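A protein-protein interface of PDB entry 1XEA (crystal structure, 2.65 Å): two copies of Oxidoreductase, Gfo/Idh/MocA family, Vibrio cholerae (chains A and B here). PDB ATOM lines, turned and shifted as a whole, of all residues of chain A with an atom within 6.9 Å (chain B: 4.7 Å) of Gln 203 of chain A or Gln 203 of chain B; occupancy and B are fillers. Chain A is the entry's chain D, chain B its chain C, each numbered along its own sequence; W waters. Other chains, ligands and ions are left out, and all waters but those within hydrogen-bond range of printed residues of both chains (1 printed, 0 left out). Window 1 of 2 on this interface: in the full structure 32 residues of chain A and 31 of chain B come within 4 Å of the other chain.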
ATOM      1  N   ARG A 148     -20.115  20.276  -3.432  1.00  0.00           N
ATOM      2  CA  ARG A 148     -19.434  20.607  -2.184  1.00  0.00           C
ATOM      3  C   ARG A 148     -19.151  19.319  -1.425  1.00  0.00           C
ATOM      4  O   ARG A 148     -20.047  18.495  -1.215  1.00  0.00           O
ATOM      5  CB  ARG A 148     -20.306  21.537  -1.329  1.00  0.00           C
ATOM      6  CG  ARG A 148     -19.666  21.997  -0.009  1.00  0.00           C
ATOM      7  CD  ARG A 148     -20.565  22.980   0.741  1.00  0.00           C
ATOM      8  NE  ARG A 148     -21.883  22.414   1.029  1.00  0.00           N
ATOM      9  CZ  ARG A 148     -23.008  23.123   1.071  1.00  0.00           C
ATOM     10  NH1 ARG A 148     -22.980  24.429   0.846  1.00  0.00           N
ATOM     11  NH2 ARG A 148     -24.164  22.523   1.321  1.00  0.00           N
ATOM     12  N   PHE A 168      -7.085  16.531   3.962  1.00  0.00           N
ATOM     13  CA  PHE A 168      -7.824  17.415   3.068  1.00  0.00           C
ATOM     14  C   PHE A 168      -7.770  16.970   1.610  1.00  0.00           C
ATOM     15  O   PHE A 168      -8.639  17.313   0.806  1.00  0.00           O
ATOM     16  CB  PHE A 168      -7.259  18.825   3.169  1.00  0.00           C
ATOM     17  CG  PHE A 168      -8.051  19.847   2.419  1.00  0.00           C
ATOM     18  CD1 PHE A 168      -9.320  20.215   2.852  1.00  0.00           C
ATOM     19  CD2 PHE A 168      -7.522  20.457   1.287  1.00  0.00           C
ATOM     20  CE1 PHE A 168     -10.049  21.178   2.172  1.00  0.00           C
ATOM     21  CE2 PHE A 168      -8.241  21.417   0.602  1.00  0.00           C
ATOM     22  CZ  PHE A 168      -9.508  21.782   1.046  1.00  0.00           C
ATOM     23  N   LEU A 172     -10.522  17.541  -1.293  1.00  0.00           N
ATOM     24  CA  LEU A 172      -9.932  18.321  -2.362  1.00  0.00           C
ATOM     25  C   LEU A 172      -9.895  17.541  -3.688  1.00  0.00           C
ATOM     26  O   LEU A 172     -10.332  18.057  -4.710  1.00  0.00           O
ATOM     27  CB  LEU A 172      -8.524  18.770  -1.980  1.00  0.00           C
ATOM     28  CG  LEU A 172      -7.866  19.744  -2.972  1.00  0.00           C
ATOM     29  CD1 LEU A 172      -8.624  21.064  -2.981  1.00  0.00           C
ATOM     30  CD2 LEU A 172      -6.408  19.989  -2.571  1.00  0.00           C
ATOM     31  N   ASP A 185      -7.529  31.919  -9.709  1.00  0.00           N
ATOM     32  CA  ASP A 185      -8.977  32.052  -9.727  1.00  0.00           C
ATOM     33  C   ASP A 185      -9.586  31.134  -8.675  1.00  0.00           C
ATOM     34  O   ASP A 185     -10.708  30.653  -8.819  1.00  0.00           O
ATOM     35  CB  ASP A 185      -9.516  31.705 -11.119  1.00  0.00           C
ATOM     36  CG  ASP A 185      -8.925  32.581 -12.210  1.00  0.00           C
ATOM     37  OD1 ASP A 185      -9.208  33.800 -12.210  1.00  0.00           O
ATOM     38  OD2 ASP A 185      -8.166  32.054 -13.061  1.00  0.00           O
ATOM     39  N   LEU A 186      -8.832  30.903  -7.609  1.00  0.00           N
ATOM     40  CA  LEU A 186      -9.276  30.042  -6.524  1.00  0.00           C
ATOM     41  C   LEU A 186      -9.432  30.839  -5.226  1.00  0.00           C
ATOM     42  O   LEU A 186      -8.733  31.831  -5.006  1.00  0.00           O
ATOM     43  CB  LEU A 186      -8.265  28.900  -6.356  1.00  0.00           C
ATOM     44  CG  LEU A 186      -8.449  27.888  -5.227  1.00  0.00           C
ATOM     45  CD1 LEU A 186      -7.891  26.527  -5.643  1.00  0.00           C
ATOM     46  CD2 LEU A 186      -7.767  28.405  -3.972  1.00  0.00           C
ATOM     47  N   HIS A 187     -10.347  30.414  -4.362  1.00  0.00           N
ATOM     48  CA  HIS A 187     -10.553  31.120  -3.105  1.00  0.00           C
ATOM     49  C   HIS A 187     -10.220  30.235  -1.905  1.00  0.00           C
ATOM     50  O   HIS A 187     -11.002  29.376  -1.509  1.00  0.00           O
ATOM     51  CB  HIS A 187     -11.994  31.614  -3.019  1.00  0.00           C
ATOM     52  CG  HIS A 187     -12.244  32.548  -1.879  1.00  0.00           C
ATOM     53  ND1 HIS A 187     -12.943  32.176  -0.751  1.00  0.00           N
ATOM     54  CD2 HIS A 187     -11.894  33.844  -1.694  1.00  0.00           C
ATOM     55  CE1 HIS A 187     -13.016  33.202   0.079  1.00  0.00           C
ATOM     56  NE2 HIS A 187     -12.387  34.226  -0.469  1.00  0.00           N
ATOM     57  N   LEU A 188      -9.048  30.464  -1.333  1.00  0.00           N
ATOM     58  CA  LEU A 188      -8.591  29.697  -0.195  1.00  0.00           C
ATOM     59  C   LEU A 188      -8.799  30.430   1.123  1.00  0.00           C
ATOM     60  O   LEU A 188      -8.264  31.519   1.325  1.00  0.00           O
ATOM     61  CB  LEU A 188      -7.106  29.379  -0.368  1.00  0.00           C
ATOM     62  CG  LEU A 188      -6.286  29.177   0.912  1.00  0.00           C
ATOM     63  CD1 LEU A 188      -6.405  27.747   1.381  1.00  0.00           C
ATOM     64  CD2 LEU A 188      -4.839  29.535   0.649  1.00  0.00           C
ATOM     65  N   THR A 189      -9.575  29.838   2.023  1.00  0.00           N
ATOM     66  CA  THR A 189      -9.796  30.456   3.324  1.00  0.00           C
ATOM     67  C   THR A 189      -9.419  29.451   4.407  1.00  0.00           C
ATOM     68  O   THR A 189      -9.372  28.252   4.138  1.00  0.00           O
ATOM     69  CB  THR A 189     -11.269  30.925   3.487  1.00  0.00           C
ATOM     70  OG1 THR A 189     -12.171  29.897   3.051  1.00  0.00           O
ATOM     71  CG2 THR A 189     -11.506  32.188   2.663  1.00  0.00           C
ATOM     72  N   ASP A 201     -10.738  25.707   3.588  1.00  0.00           N
ATOM     73  CA  ASP A 201     -11.788  25.864   2.593  1.00  0.00           C
ATOM     74  C   ASP A 201     -11.216  26.325   1.262  1.00  0.00           C
ATOM     75  O   ASP A 201     -10.709  27.438   1.143  1.00  0.00           O
ATOM     76  CB  ASP A 201     -12.835  26.877   3.073  1.00  0.00           C
ATOM     77  CG  ASP A 201     -13.998  26.223   3.810  1.00  0.00           C
ATOM     78  OD1 ASP A 201     -14.903  25.669   3.137  1.00  0.00           O
ATOM     79  OD2 ASP A 201     -14.006  26.263   5.063  1.00  0.00           O
ATOM     80  N   VAL A 202     -11.298  25.449   0.271  1.00  0.00           N
ATOM     81  CA  VAL A 202     -10.831  25.743  -1.070  1.00  0.00           C
ATOM     82  C   VAL A 202     -12.053  25.625  -1.964  1.00  0.00           C
ATOM     83  O   VAL A 202     -12.733  24.599  -1.980  1.00  0.00           O
ATOM     84  CB  VAL A 202      -9.782  24.747  -1.514  1.00  0.00           C
ATOM     85  CG1 VAL A 202      -9.557  24.861  -3.008  1.00  0.00           C
ATOM     86  CG2 VAL A 202      -8.516  25.002  -0.763  1.00  0.00           C
ATOM     87  N   GLN A 203     -12.327  26.685  -2.706  1.00  0.00           N
ATOM     88  CA  GLN A 203     -13.481  26.723  -3.576  1.00  0.00           C
ATOM     89  C   GLN A 203     -13.149  27.525  -4.830  1.00  0.00           C
ATOM     90  O   GLN A 203     -12.489  28.561  -4.756  1.00  0.00           O
ATOM     91  CB  GLN A 203     -14.644  27.354  -2.806  1.00  0.00           C
ATOM     92  CG  GLN A 203     -15.641  28.121  -3.648  1.00  0.00           C
ATOM     93  CD  GLN A 203     -16.740  28.807  -2.828  1.00  0.00           C
ATOM     94  OE1 GLN A 203     -17.217  29.888  -3.197  1.00  0.00           O
ATOM     95  NE2 GLN A 203     -17.155  28.177  -1.731  1.00  0.00           N
ATOM     96  N   TRP A 204     -13.600  27.040  -5.981  1.00  0.00           N
ATOM     97  CA  TRP A 204     -13.344  27.729  -7.240  1.00  0.00           C
ATOM     98  C   TRP A 204     -14.396  27.372  -8.278  1.00  0.00           C
ATOM     99  O   TRP A 204     -15.144  26.410  -8.115  1.00  0.00           O
ATOM    100  CB  TRP A 204     -11.964  27.354  -7.764  1.00  0.00           C
ATOM    101  CG  TRP A 204     -11.867  25.953  -8.286  1.00  0.00           C
ATOM    102  CD1 TRP A 204     -12.062  25.540  -9.575  1.00  0.00           C
ATOM    103  CD2 TRP A 204     -11.461  24.798  -7.553  1.00  0.00           C
ATOM    104  NE1 TRP A 204     -11.786  24.199  -9.691  1.00  0.00           N
ATOM    105  CE2 TRP A 204     -11.414  23.719  -8.462  1.00  0.00           C
ATOM    106  CE3 TRP A 204     -11.125  24.568  -6.211  1.00  0.00           C
ATOM    107  CZ2 TRP A 204     -11.037  22.429  -8.076  1.00  0.00           C
ATOM    108  CZ3 TRP A 204     -10.753  23.286  -5.829  1.00  0.00           C
ATOM    109  CH2 TRP A 204     -10.712  22.233  -6.761  1.00  0.00           C
ATOM    110  N   GLN A 205     -14.454  28.146  -9.354  1.00  0.00           N
ATOM    111  CA  GLN A 205     -15.429  27.874 -10.399  1.00  0.00           C
ATOM    112  C   GLN A 205     -14.831  27.811 -11.800  1.00  0.00           C
ATOM    113  O   GLN A 205     -14.333  28.804 -12.328  1.00  0.00           O
ATOM    114  CB  GLN A 205     -16.550  28.915 -10.363  1.00  0.00           C
ATOM    115  CG  GLN A 205     -17.457  28.874 -11.586  1.00  0.00           C
ATOM    116  CD  GLN A 205     -18.824  29.476 -11.327  1.00  0.00           C
ATOM    117  OE1 GLN A 205     -18.961  30.436 -10.563  1.00  0.00           O
ATOM    118  NE2 GLN A 205     -19.843  28.921 -11.975  1.00  0.00           N
ATOM    119  N   LEU A 210     -19.347  24.992  -9.828  1.00  0.00           N
ATOM    120  CA  LEU A 210     -18.695  25.535  -8.639  1.00  0.00           C
ATOM    121  C   LEU A 210     -18.265  24.357  -7.772  1.00  0.00           C
ATOM    122  O   LEU A 210     -19.104  23.645  -7.220  1.00  0.00           O
ATOM    123  CB  LEU A 210     -19.658  26.430  -7.853  1.00  0.00           C
ATOM    124  CG  LEU A 210     -19.118  26.929  -6.509  1.00  0.00           C
ATOM    125  CD1 LEU A 210     -17.912  27.823  -6.734  1.00  0.00           C
ATOM    126  CD2 LEU A 210     -20.208  27.680  -5.762  1.00  0.00           C
ATOM    127  N   LEU A 211     -16.955  24.152  -7.676  1.00  0.00           N
ATOM    128  CA  LEU A 211     -16.380  23.065  -6.892  1.00  0.00           C
ATOM    129  C   LEU A 211     -15.917  23.594  -5.535  1.00  0.00           C
ATOM    130  O   LEU A 211     -15.251  24.625  -5.448  1.00  0.00           O
ATOM    131  CB  LEU A 211     -15.210  22.447  -7.660  1.00  0.00           C
ATOM    132  CG  LEU A 211     -15.523  21.998  -9.101  1.00  0.00           C
ATOM    133  CD1 LEU A 211     -14.254  21.510  -9.787  1.00  0.00           C
ATOM    134  CD2 LEU A 211     -16.569  20.906  -9.085  1.00  0.00           C
ATOM    135  N   HIS A 212     -16.249  22.874  -4.473  1.00  0.00           N
ATOM    136  CA  HIS A 212     -15.913  23.333  -3.134  1.00  0.00           C
ATOM    137  C   HIS A 212     -15.459  22.188  -2.226  1.00  0.00           C
ATOM    138  O   HIS A 212     -16.179  21.199  -2.061  1.00  0.00           O
ATOM    139  CB  HIS A 212     -17.159  24.022  -2.571  1.00  0.00           C
ATOM    140  CG  HIS A 212     -16.963  24.675  -1.243  1.00  0.00           C
ATOM    141  ND1 HIS A 212     -18.002  25.265  -0.556  1.00  0.00           N
ATOM    142  CD2 HIS A 212     -15.862  24.839  -0.476  1.00  0.00           C
ATOM    143  CE1 HIS A 212     -17.549  25.762   0.581  1.00  0.00           C
ATOM    144  NE2 HIS A 212     -16.253  25.517   0.654  1.00  0.00           N
ATOM    145  N   ALA A 213     -14.264  22.330  -1.651  1.00  0.00           N
ATOM    146  CA  ALA A 213     -13.703  21.332  -0.735  1.00  0.00           C
ATOM    147  C   ALA A 213     -13.598  21.964   0.646  1.00  0.00           C
ATOM    148  O   ALA A 213     -12.937  22.987   0.822  1.00  0.00           O
ATOM    149  CB  ALA A 213     -12.339  20.880  -1.212  1.00  0.00           C
ATOM    150  N   LEU B 186     -13.578  39.543  -1.213  1.00  0.00           N
ATOM    151  CA  LEU B 186     -14.796  38.756  -1.194  1.00  0.00           C
ATOM    152  C   LEU B 186     -14.872  37.906  -2.447  1.00  0.00           C
ATOM    153  O   LEU B 186     -14.449  38.336  -3.512  1.00  0.00           O
ATOM    154  CB  LEU B 186     -15.993  39.702  -1.108  1.00  0.00           C
ATOM    155  CG  LEU B 186     -17.400  39.106  -1.083  1.00  0.00           C
ATOM    156  CD1 LEU B 186     -18.355  40.128  -0.489  1.00  0.00           C
ATOM    157  CD2 LEU B 186     -17.833  38.700  -2.491  1.00  0.00           C
ATOM    158  N   HIS B 187     -15.394  36.696  -2.325  1.00  0.00           N
ATOM    159  CA  HIS B 187     -15.505  35.823  -3.483  1.00  0.00           C
ATOM    160  C   HIS B 187     -16.952  35.830  -3.945  1.00  0.00           C
ATOM    161  O   HIS B 187     -17.875  35.707  -3.135  1.00  0.00           O
ATOM    162  CB  HIS B 187     -15.082  34.403  -3.118  1.00  0.00           C
ATOM    163  CG  HIS B 187     -14.774  33.535  -4.300  1.00  0.00           C
ATOM    164  ND1 HIS B 187     -15.422  32.340  -4.536  1.00  0.00           N
ATOM    165  CD2 HIS B 187     -13.849  33.659  -5.281  1.00  0.00           C
ATOM    166  CE1 HIS B 187     -14.907  31.766  -5.610  1.00  0.00           C
ATOM    167  NE2 HIS B 187     -13.951  32.546  -6.081  1.00  0.00           N
ATOM    168  N   THR B 189     -19.462  34.106  -6.961  1.00  0.00           N
ATOM    169  CA  THR B 189     -19.653  33.201  -8.088  1.00  0.00           C
ATOM    170  C   THR B 189     -21.146  33.161  -8.385  1.00  0.00           C
ATOM    171  O   THR B 189     -21.969  33.332  -7.484  1.00  0.00           O
ATOM    172  CB  THR B 189     -19.140  31.755  -7.803  1.00  0.00           C
ATOM    173  OG1 THR B 189     -19.684  31.270  -6.569  1.00  0.00           O
ATOM    174  CG2 THR B 189     -17.623  31.725  -7.746  1.00  0.00           C
ATOM    175  N   ASP B 201     -23.565  32.819  -5.263  1.00  0.00           N
ATOM    176  CA  ASP B 201     -22.843  32.393  -4.071  1.00  0.00           C
ATOM    177  C   ASP B 201     -21.845  33.474  -3.684  1.00  0.00           C
ATOM    178  O   ASP B 201     -20.934  33.780  -4.446  1.00  0.00           O
ATOM    179  CB  ASP B 201     -22.122  31.066  -4.340  1.00  0.00           C
ATOM    180  CG  ASP B 201     -23.075  29.864  -4.353  1.00  0.00           C
ATOM    181  OD1 ASP B 201     -23.277  29.229  -3.282  1.00  0.00           O
ATOM    182  OD2 ASP B 201     -23.628  29.556  -5.432  1.00  0.00           O
ATOM    183  N   VAL B 202     -22.020  34.055  -2.503  1.00  0.00           N
ATOM    184  CA  VAL B 202     -21.130  35.109  -2.041  1.00  0.00           C
ATOM    185  C   VAL B 202     -20.550  34.786  -0.679  1.00  0.00           C
ATOM    186  O   VAL B 202     -21.286  34.555   0.279  1.00  0.00           O
ATOM    187  CB  VAL B 202     -21.882  36.462  -1.952  1.00  0.00           C
ATOM    188  CG1 VAL B 202     -21.006  37.525  -1.292  1.00  0.00           C
ATOM    189  CG2 VAL B 202     -22.300  36.903  -3.339  1.00  0.00           C
ATOM    190  N   GLN B 203     -19.227  34.768  -0.586  1.00  0.00           N
ATOM    191  CA  GLN B 203     -18.593  34.500   0.697  1.00  0.00           C
ATOM    192  C   GLN B 203     -17.265  35.225   0.902  1.00  0.00           C
ATOM    193  O   GLN B 203     -16.499  35.428  -0.040  1.00  0.00           O
ATOM    194  CB  GLN B 203     -18.390  32.997   0.895  1.00  0.00           C
ATOM    195  CG  GLN B 203     -17.578  32.297  -0.163  1.00  0.00           C
ATOM    196  CD  GLN B 203     -16.921  31.040   0.381  1.00  0.00           C
ATOM    197  OE1 GLN B 203     -15.943  31.129   1.121  1.00  0.00           O
ATOM    198  NE2 GLN B 203     -17.466  29.865   0.038  1.00  0.00           N
ATOM    199  N   TRP B 204     -16.998  35.604   2.147  1.00  0.00           N
ATOM    200  CA  TRP B 204     -15.764  36.289   2.486  1.00  0.00           C
ATOM    201  C   TRP B 204     -15.362  35.991   3.931  1.00  0.00           C
ATOM    202  O   TRP B 204     -16.174  35.509   4.732  1.00  0.00           O
ATOM    203  CB  TRP B 204     -15.942  37.787   2.303  1.00  0.00           C
ATOM    204  CG  TRP B 204     -16.873  38.387   3.299  1.00  0.00           C
ATOM    205  CD1 TRP B 204     -16.538  39.087   4.420  1.00  0.00           C
ATOM    206  CD2 TRP B 204     -18.302  38.391   3.231  1.00  0.00           C
ATOM    207  NE1 TRP B 204     -17.672  39.542   5.051  1.00  0.00           N
ATOM    208  CE2 TRP B 204     -18.766  39.130   4.344  1.00  0.00           C
ATOM    209  CE3 TRP B 204     -19.232  37.845   2.336  1.00  0.00           C
ATOM    210  CZ2 TRP B 204     -20.125  39.340   4.579  1.00  0.00           C
ATOM    211  CZ3 TRP B 204     -20.577  38.053   2.570  1.00  0.00           C
ATOM    212  CH2 TRP B 204     -21.011  38.797   3.685  1.00  0.00           C
ATOM    213  N   LEU B 210     -15.752  33.046   8.656  1.00  0.00           N
ATOM    214  CA  LEU B 210     -16.033  32.908   7.232  1.00  0.00           C
ATOM    215  C   LEU B 210     -17.535  33.027   7.001  1.00  0.00           C
ATOM    216  O   LEU B 210     -18.296  32.123   7.363  1.00  0.00           O
ATOM    217  CB  LEU B 210     -15.535  31.552   6.732  1.00  0.00           C
ATOM    218  CG  LEU B 210     -15.725  31.240   5.247  1.00  0.00           C
ATOM    219  CD1 LEU B 210     -14.886  32.184   4.387  1.00  0.00           C
ATOM    220  CD2 LEU B 210     -15.330  29.802   4.997  1.00  0.00           C
ATOM    221  N   LEU B 211     -17.957  34.141   6.404  1.00  0.00           N
ATOM    222  CA  LEU B 211     -19.383  34.385   6.124  1.00  0.00           C
ATOM    223  C   LEU B 211     -19.751  33.898   4.721  1.00  0.00           C
ATOM    224  O   LEU B 211     -18.994  34.105   3.785  1.00  0.00           O
ATOM    225  CB  LEU B 211     -19.687  35.879   6.273  1.00  0.00           C
ATOM    226  CG  LEU B 211     -19.288  36.438   7.642  1.00  0.00           C
ATOM    227  CD1 LEU B 211     -19.645  37.909   7.733  1.00  0.00           C
ATOM    228  CD2 LEU B 211     -20.006  35.657   8.727  1.00  0.00           C
ATOM    229  N   HIS B 212     -20.909  33.259   4.568  1.00  0.00           N
ATOM    230  CA  HIS B 212     -21.307  32.730   3.259  1.00  0.00           C
ATOM    231  C   HIS B 212     -22.813  32.725   2.996  1.00  0.00           C
ATOM    232  O   HIS B 212     -23.591  32.056   3.696  1.00  0.00           O
ATOM    233  CB  HIS B 212     -20.751  31.304   3.100  1.00  0.00           C
ATOM    234  CG  HIS B 212     -21.044  30.660   1.776  1.00  0.00           C
ATOM    235  ND1 HIS B 212     -20.641  29.374   1.476  1.00  0.00           N
ATOM    236  CD2 HIS B 212     -21.687  31.115   0.673  1.00  0.00           C
ATOM    237  CE1 HIS B 212     -21.023  29.067   0.250  1.00  0.00           C
ATOM    238  NE2 HIS B 212     -21.660  30.105  -0.259  1.00  0.00           N
HETATM  239  O   HOH W   1     -13.492  31.092  -8.560  1.00  0.00           O
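ND1 of His 187 of chain B lies within hydrogen-bond range of OE1 of Gln 203 of chain A (3.3 Å). NE2 of Gln 203 of chain B sits close to NE2 of Gln 203 of chain A (2.5 Å).
N of Thr 189 of chain A is in hydrogen-bond range of O of Asp 201 of chain A, at 2.8 Å. O of Gln 203 of chain B is in hydrogen-bond range of N of His 187 of chain B, 2.8 Å away. O of Gln 203 of chain A is in hydrogen-bond range of N of His 187 of chain A (2.9 Å). The side-chain carboxylate (OD1) of Asp 201 of chain A sits at hydrogen-bond distance from a ring nitrogen (NE2) of His 212 of chain A, 2.8 Å away. ND1 of His 212 of chain A lies within hydrogen-bond range of NE2 of Gln 203 of chain A, 3.3 Å away. The backbone carbonyl oxygen (O) of Thr 189 of chain B is in hydrogen-bond range of the backbone NH (N) of Asp 201 of chain B (2.8 Å).
His 187 of chain B touches His 187 of chain A. His 187 of chain A touches Gln 203 of chain B. Thr 189 of chain A touches Leu 210 of chain B (OG1 to CD2, 3.7 Å). OD2 of Asp 201 of chain A touches CD2 of Leu 210 of chain B, at 3.8 Å. OE1 of Gln 205 of chain A touches CB of Thr 189 of chain B, at 3.1 Å. CD2 of Leu 210 of chain A touches OG1 of Thr 189 of chain B, at 3.7 Å. CD2 of Leu 210 of chain A touches CG of Asp 201 of chain B (3.9 Å).
Printed residues of chain B within 4 Å of Gln 203 of chain A: His 187 (3.3 Å) and Gln 203 (2.5 Å). Of the printed residues of chain A, Gln 203 of chain B touches His 187 (3.7 Å) and Gln 203 (2.5 Å). Of the printed residues of chain B, Leu 210 of chain A touches Thr 189 and Asp 201. Of the printed residues of chain B, Thr 189 of chain A touches Leu 210 (3.7 Å). Printed residues of chain B within 4 Å of Gln 205 of chain A: Thr 189. Of the printed residues of chain A, His 187 of chain B touches His 187 and Gln 203. Printed residues of chain A within 4 Å of Leu 210 of chain B: Thr 189 and Asp 201. His 212 of chain B touches none of the printed residues of chain A. Trp 204 of chain B touches none of the printed residues of chain A. The nearest residue of chain A that does not touch Gln 203 of chain B is His 212 of chain A (4.1 Å). The nearest printed residue of chain A that does not touch Thr 189 of chain B is Gln 203 of chain A (4.4 Å).
Printed residues of chain A that touch a printed residue of chain B: His 187, Thr 189, Asp 201, Gln 203, Gln 205 and Leu 210. Hydrophobic or aromatic side chains of chain B that line the printed part of chain A: His 187 and Leu 210. Among the printed residues, 9 pairs touch across the chains. Among the printed residues, no Asp or Glu carboxylate lies within 4 Å of a Lys or Arg side-chain nitrogen of the other chain.
His 187 of chain A touches its own counterpart, His 187 of chain B. His 187 of chain A touches Gln 203 of chain B, and with the chains exchanged Gln 203 of chain A touches His 187 of chain B. Thr 189 of chain A touches Leu 210 of chain B, and with the chains exchanged Leu 210 of chain A touches Thr 189 of chain B. Asp 201 of chain A touches Leu 210 of chain B, and with the chains exchanged Leu 210 of chain A touches Asp 201 of chain B. Positions printed for both chains: 186, 187, 189, 201, 202, 203, 204, 210, 211 and 212.
Water W1 lies within hydrogen-bond range of O of Asp 185 of chain A, NE2 of His 187 of chain B and N of Gln 205 of chain A.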
